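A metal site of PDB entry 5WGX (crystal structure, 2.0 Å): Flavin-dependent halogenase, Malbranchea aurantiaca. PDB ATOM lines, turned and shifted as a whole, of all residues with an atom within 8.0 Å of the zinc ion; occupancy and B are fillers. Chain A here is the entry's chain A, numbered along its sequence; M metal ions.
N of Ser 615 sits close to SG of Cys 613.
N of Cys 613 sits at hydrogen-bond distance from O of Leu 618, 2.8 Å away.
SG of Cys 600 lies close to N of Ala 602, 3.4 Å away.
SG of Cys 597 lies close to N of Gly 599, 3.4 Å away.
The backbone NH of Cys 597 sits at hydrogen-bond distance from the backbone carbonyl oxygen of Ala 602.
The backbone NH (N) of Leu 618 lies close to the side-chain sulfur (SG) of Cys 616, 3.4 Å away.
Along chain A the residues within 4 Å of the zinc ion span positions 597 to 616.
The zinc ion is bound by SG of Cys 616, SG of Cys 613, SG of Cys 600 and SG of Cys 597.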
ATOM      1  N   ARG A 268       9.613  -8.832   3.172  1.00  0.00           N
ATOM      2  CA  ARG A 268       8.669  -7.750   2.995  1.00  0.00           C
ATOM      3  C   ARG A 268       7.459  -8.252   2.202  1.00  0.00           C
ATOM      4  O   ARG A 268       7.630  -8.790   1.094  1.00  0.00           O
ATOM      5  CB  ARG A 268       9.336  -6.567   2.277  1.00  0.00           C
ATOM      6  CG  ARG A 268       8.424  -5.360   2.096  1.00  0.00           C
ATOM      7  CD  ARG A 268       8.977  -4.354   1.085  1.00  0.00           C
ATOM      8  NE  ARG A 268       7.887  -3.558   0.505  1.00  0.00           N
ATOM      9  CZ  ARG A 268       7.573  -2.327   0.863  1.00  0.00           C
ATOM     10  NH1 ARG A 268       8.274  -1.694   1.798  1.00  0.00           N
ATOM     11  NH2 ARG A 268       6.561  -1.703   0.272  1.00  0.00           N
ATOM     12  N   SER A 302      -4.982  -1.855  -8.890  1.00  0.00           N
ATOM     13  CA  SER A 302      -3.870  -2.068  -7.984  1.00  0.00           C
ATOM     14  C   SER A 302      -4.359  -2.702  -6.692  1.00  0.00           C
ATOM     15  O   SER A 302      -5.561  -2.752  -6.403  1.00  0.00           O
ATOM     16  CB  SER A 302      -3.140  -0.761  -7.688  1.00  0.00           C
ATOM     17  OG  SER A 302      -3.929   0.077  -6.849  1.00  0.00           O
ATOM     18  N   GLU A 304      -4.177  -1.624  -3.622  1.00  0.00           N
ATOM     19  CA  GLU A 304      -4.944  -0.689  -2.794  1.00  0.00           C
ATOM     20  C   GLU A 304      -6.319  -0.410  -3.386  1.00  0.00           C
ATOM     21  O   GLU A 304      -7.291  -0.236  -2.630  1.00  0.00           O
ATOM     22  CB  GLU A 304      -4.166   0.615  -2.613  1.00  0.00           C
ATOM     23  CG  GLU A 304      -2.860   0.447  -1.845  1.00  0.00           C
ATOM     24  CD  GLU A 304      -2.093   1.750  -1.698  1.00  0.00           C
ATOM     25  OE1 GLU A 304      -2.658   2.818  -2.007  1.00  0.00           O
ATOM     26  OE2 GLU A 304      -0.910   1.703  -1.287  1.00  0.00           O
ATOM     27  N   TRP A 316       1.501  -2.908   4.503  1.00  0.00           N
ATOM     28  CA  TRP A 316       2.816  -3.503   4.279  1.00  0.00           C
ATOM     29  C   TRP A 316       3.460  -3.843   5.624  1.00  0.00           C
ATOM     30  O   TRP A 316       3.473  -3.015   6.538  1.00  0.00           O
ATOM     31  CB  TRP A 316       3.718  -2.543   3.492  1.00  0.00           C
ATOM     32  CG  TRP A 316       3.405  -2.551   2.028  1.00  0.00           C
ATOM     33  CD1 TRP A 316       2.698  -1.620   1.342  1.00  0.00           C
ATOM     34  CD2 TRP A 316       3.787  -3.557   1.091  1.00  0.00           C
ATOM     35  NE1 TRP A 316       2.617  -1.973   0.011  1.00  0.00           N
ATOM     36  CE2 TRP A 316       3.284  -3.160  -0.166  1.00  0.00           C
ATOM     37  CE3 TRP A 316       4.510  -4.749   1.176  1.00  0.00           C
ATOM     38  CZ2 TRP A 316       3.465  -3.923  -1.325  1.00  0.00           C
ATOM     39  CZ3 TRP A 316       4.699  -5.497   0.032  1.00  0.00           C
ATOM     40  CH2 TRP A 316       4.182  -5.082  -1.202  1.00  0.00           C
ATOM     41  N   ARG A 595      12.506  -1.909  -9.041  1.00  0.00           N
ATOM     42  CA  ARG A 595      12.609  -0.572  -8.489  1.00  0.00           C
ATOM     43  C   ARG A 595      11.512  -0.399  -7.456  1.00  0.00           C
ATOM     44  O   ARG A 595      10.526  -1.132  -7.438  1.00  0.00           O
ATOM     45  CB  ARG A 595      12.482   0.509  -9.565  1.00  0.00           C
ATOM     46  CG  ARG A 595      11.048   0.715 -10.033  1.00  0.00           C
ATOM     47  CD  ARG A 595      10.914   1.898 -10.983  1.00  0.00           C
ATOM     48  NE  ARG A 595       9.519   2.071 -11.395  1.00  0.00           N
ATOM     49  CZ  ARG A 595       8.663   2.898 -10.807  1.00  0.00           C
ATOM     50  NH1 ARG A 595       9.053   3.638  -9.771  1.00  0.00           N
ATOM     51  NH2 ARG A 595       7.418   2.990 -11.248  1.00  0.00           N
ATOM     52  N   GLN A 596      11.709   0.583  -6.583  1.00  0.00           N
ATOM     53  CA  GLN A 596      10.753   0.900  -5.527  1.00  0.00           C
ATOM     54  C   GLN A 596       9.829   2.014  -5.979  1.00  0.00           C
ATOM     55  O   GLN A 596      10.295   3.032  -6.510  1.00  0.00           O
ATOM     56  CB  GLN A 596      11.478   1.307  -4.246  1.00  0.00           C
ATOM     57  CG  GLN A 596      11.049   0.537  -3.022  1.00  0.00           C
ATOM     58  CD  GLN A 596      11.675   1.051  -1.738  1.00  0.00           C
ATOM     59  OE1 GLN A 596      12.772   1.605  -1.750  1.00  0.00           O
ATOM     60  NE2 GLN A 596      10.969   0.887  -0.631  1.00  0.00           N
ATOM     61  N   CYS A 597       8.527   1.829  -5.798  1.00  0.00           N
ATOM     62  CA  CYS A 597       7.571   2.887  -6.089  1.00  0.00           C
ATOM     63  C   CYS A 597       7.828   4.070  -5.183  1.00  0.00           C
ATOM     64  O   CYS A 597       7.903   3.935  -3.955  1.00  0.00           O
ATOM     65  CB  CYS A 597       6.146   2.379  -5.915  1.00  0.00           C
ATOM     66  SG  CYS A 597       4.860   3.618  -6.242  1.00  0.00           S
ATOM     67  N   SER A 598       7.986   5.255  -5.776  1.00  0.00           N
ATOM     68  CA  SER A 598       8.229   6.455  -4.986  1.00  0.00           C
ATOM     69  C   SER A 598       7.022   6.852  -4.161  1.00  0.00           C
ATOM     70  O   SER A 598       7.172   7.549  -3.152  1.00  0.00           O
ATOM     71  CB  SER A 598       8.654   7.614  -5.883  1.00  0.00           C
ATOM     72  OG  SER A 598       7.639   7.928  -6.825  1.00  0.00           O
ATOM     73  N   GLY A 599       5.827   6.413  -4.549  1.00  0.00           N
ATOM     74  CA  GLY A 599       4.611   6.762  -3.835  1.00  0.00           C
ATOM     75  C   GLY A 599       4.358   5.933  -2.594  1.00  0.00           C
ATOM     76  O   GLY A 599       4.176   6.479  -1.504  1.00  0.00           O
ATOM     77  N   CYS A 600       4.364   4.602  -2.749  1.00  0.00           N
ATOM     78  CA  CYS A 600       3.962   3.705  -1.671  1.00  0.00           C
ATOM     79  C   CYS A 600       5.091   2.838  -1.140  1.00  0.00           C
ATOM     80  O   CYS A 600       4.899   2.165  -0.121  1.00  0.00           O
ATOM     81  CB  CYS A 600       2.813   2.806  -2.141  1.00  0.00           C
ATOM     82  SG  CYS A 600       3.342   1.507  -3.282  1.00  0.00           S
ATOM     83  N   GLY A 601       6.251   2.808  -1.802  1.00  0.00           N
ATOM     84  CA  GLY A 601       7.362   1.997  -1.365  1.00  0.00           C
ATOM     85  C   GLY A 601       7.359   0.559  -1.841  1.00  0.00           C
ATOM     86  O   GLY A 601       8.327  -0.167  -1.563  1.00  0.00           O
ATOM     87  N   ALA A 602       6.322   0.121  -2.551  1.00  0.00           N
ATOM     88  CA  ALA A 602       6.265  -1.266  -2.990  1.00  0.00           C
ATOM     89  C   ALA A 602       7.287  -1.522  -4.104  1.00  0.00           C
ATOM     90  O   ALA A 602       7.500  -0.688  -4.986  1.00  0.00           O
ATOM     91  CB  ALA A 602       4.871  -1.623  -3.490  1.00  0.00           C
ATOM     92  N   TRP A 603       7.908  -2.705  -4.051  1.00  0.00           N
ATOM     93  CA  TRP A 603       8.882  -3.067  -5.067  1.00  0.00           C
ATOM     94  C   TRP A 603       8.177  -3.609  -6.313  1.00  0.00           C
ATOM     95  O   TRP A 603       7.207  -4.368  -6.221  1.00  0.00           O
ATOM     96  CB  TRP A 603       9.855  -4.104  -4.509  1.00  0.00           C
ATOM     97  CG  TRP A 603      10.848  -3.481  -3.560  1.00  0.00           C
ATOM     98  CD1 TRP A 603      10.684  -3.279  -2.215  1.00  0.00           C
ATOM     99  CD2 TRP A 603      12.147  -2.973  -3.889  1.00  0.00           C
ATOM    100  NE1 TRP A 603      11.806  -2.685  -1.689  1.00  0.00           N
ATOM    101  CE2 TRP A 603      12.713  -2.491  -2.692  1.00  0.00           C
ATOM    102  CE3 TRP A 603      12.886  -2.888  -5.076  1.00  0.00           C
ATOM    103  CZ2 TRP A 603      13.987  -1.917  -2.653  1.00  0.00           C
ATOM    104  CZ3 TRP A 603      14.152  -2.319  -5.034  1.00  0.00           C
ATOM    105  CH2 TRP A 603      14.688  -1.840  -3.825  1.00  0.00           C
ATOM    106  N   LEU A 604       8.678  -3.198  -7.470  1.00  0.00           N
ATOM    107  CA  LEU A 604       8.021  -3.422  -8.755  1.00  0.00           C
ATOM    108  C   LEU A 604       8.989  -4.104  -9.719  1.00  0.00           C
ATOM    109  O   LEU A 604      10.197  -3.890  -9.662  1.00  0.00           O
ATOM    110  CB  LEU A 604       7.540  -2.100  -9.367  1.00  0.00           C
ATOM    111  CG  LEU A 604       6.775  -1.162  -8.423  1.00  0.00           C
ATOM    112  CD1 LEU A 604       6.596   0.220  -9.040  1.00  0.00           C
ATOM    113  CD2 LEU A 604       5.423  -1.771  -8.070  1.00  0.00           C
ATOM    114  N   LYS A 612       2.474   1.444 -14.505  1.00  0.00           N
ATOM    115  CA  LYS A 612       1.959   1.871 -13.212  1.00  0.00           C
ATOM    116  C   LYS A 612       2.354   0.882 -12.114  1.00  0.00           C
ATOM    117  O   LYS A 612       2.503  -0.319 -12.366  1.00  0.00           O
ATOM    118  CB  LYS A 612       0.433   2.030 -13.244  1.00  0.00           C
ATOM    119  CG  LYS A 612      -0.327   0.707 -13.157  1.00  0.00           C
ATOM    120  CD  LYS A 612      -1.828   0.934 -12.996  1.00  0.00           C
ATOM    121  CE  LYS A 612      -2.546  -0.382 -12.702  1.00  0.00           C
ATOM    122  NZ  LYS A 612      -4.024  -0.193 -12.541  1.00  0.00           N
ATOM    123  N   CYS A 613       2.521   1.403 -10.905  1.00  0.00           N
ATOM    124  CA  CYS A 613       2.728   0.561  -9.737  1.00  0.00           C
ATOM    125  C   CYS A 613       1.550  -0.388  -9.560  1.00  0.00           C
ATOM    126  O   CYS A 613       0.401   0.039  -9.545  1.00  0.00           O
ATOM    127  CB  CYS A 613       2.917   1.426  -8.490  1.00  0.00           C
ATOM    128  SG  CYS A 613       2.981   0.515  -6.899  1.00  0.00           S
ATOM    129  N   HIS A 614       1.852  -1.687  -9.434  1.00  0.00           N
ATOM    130  CA  HIS A 614       0.795  -2.673  -9.289  1.00  0.00           C
ATOM    131  C   HIS A 614       0.156  -2.647  -7.897  1.00  0.00           C
ATOM    132  O   HIS A 614      -0.886  -3.276  -7.710  1.00  0.00           O
ATOM    133  CB  HIS A 614       1.334  -4.086  -9.567  1.00  0.00           C
ATOM    134  CG  HIS A 614       2.266  -4.598  -8.508  1.00  0.00           C
ATOM    135  ND1 HIS A 614       3.628  -4.554  -8.626  1.00  0.00           N
ATOM    136  CD2 HIS A 614       2.005  -5.155  -7.304  1.00  0.00           C
ATOM    137  CE1 HIS A 614       4.183  -5.072  -7.539  1.00  0.00           C
ATOM    138  NE2 HIS A 614       3.222  -5.442  -6.723  1.00  0.00           N
ATOM    139  N   SER A 615       0.763  -1.947  -6.936  1.00  0.00           N
ATOM    140  CA  SER A 615       0.283  -1.934  -5.567  1.00  0.00           C
ATOM    141  C   SER A 615      -0.597  -0.724  -5.258  1.00  0.00           C
ATOM    142  O   SER A 615      -1.632  -0.884  -4.606  1.00  0.00           O
ATOM    143  CB  SER A 615       1.464  -1.962  -4.595  1.00  0.00           C
ATOM    144  OG  SER A 615       1.045  -2.395  -3.306  1.00  0.00           O
ATOM    145  N   CYS A 616      -0.210   0.471  -5.699  1.00  0.00           N
ATOM    146  CA  CYS A 616      -0.987   1.671  -5.428  1.00  0.00           C
ATOM    147  C   CYS A 616      -1.490   2.371  -6.682  1.00  0.00           C
ATOM    148  O   CYS A 616      -2.277   3.326  -6.555  1.00  0.00           O
ATOM    149  CB  CYS A 616      -0.149   2.674  -4.608  1.00  0.00           C
ATOM    150  SG  CYS A 616       1.050   3.600  -5.589  1.00  0.00           S
ATOM    151  N   GLY A 617      -1.078   1.949  -7.876  1.00  0.00           N
ATOM    152  CA  GLY A 617      -1.573   2.530  -9.104  1.00  0.00           C
ATOM    153  C   GLY A 617      -0.817   3.747  -9.607  1.00  0.00           C
ATOM    154  O   GLY A 617      -1.118   4.227 -10.699  1.00  0.00           O
ATOM    155  N   LEU A 618       0.151   4.248  -8.843  1.00  0.00           N
ATOM    156  CA  LEU A 618       0.873   5.446  -9.265  1.00  0.00           C
ATOM    157  C   LEU A 618       1.661   5.181 -10.544  1.00  0.00           C
ATOM    158  O   LEU A 618       2.384   4.198 -10.655  1.00  0.00           O
ATOM    159  CB  LEU A 618       1.820   5.915  -8.155  1.00  0.00           C
ATOM    160  CG  LEU A 618       2.780   7.054  -8.523  1.00  0.00           C
ATOM    161  CD1 LEU A 618       2.013   8.297  -8.932  1.00  0.00           C
ATOM    162  CD2 LEU A 618       3.718   7.345  -7.365  1.00  0.00           C
ATOM    163  N   LEU A 619       1.511   6.086 -11.502  1.00  0.00           N
ATOM    164  CA  LEU A 619       2.167   5.951 -12.792  1.00  0.00           C
ATOM    165  C   LEU A 619       3.644   6.335 -12.679  1.00  0.00           C
ATOM    166  O   LEU A 619       3.972   7.386 -12.124  1.00  0.00           O
ATOM    167  CB  LEU A 619       1.468   6.805 -13.841  1.00  0.00           C
ATOM    168  CG  LEU A 619       1.762   6.504 -15.309  1.00  0.00           C
ATOM    169  CD1 LEU A 619       1.232   5.125 -15.684  1.00  0.00           C
ATOM    170  CD2 LEU A 619       1.177   7.571 -16.215  1.00  0.00           C
HETATM  171 ZN    ZN M   1       2.984   2.370  -5.459  1.00  0.00          ZN
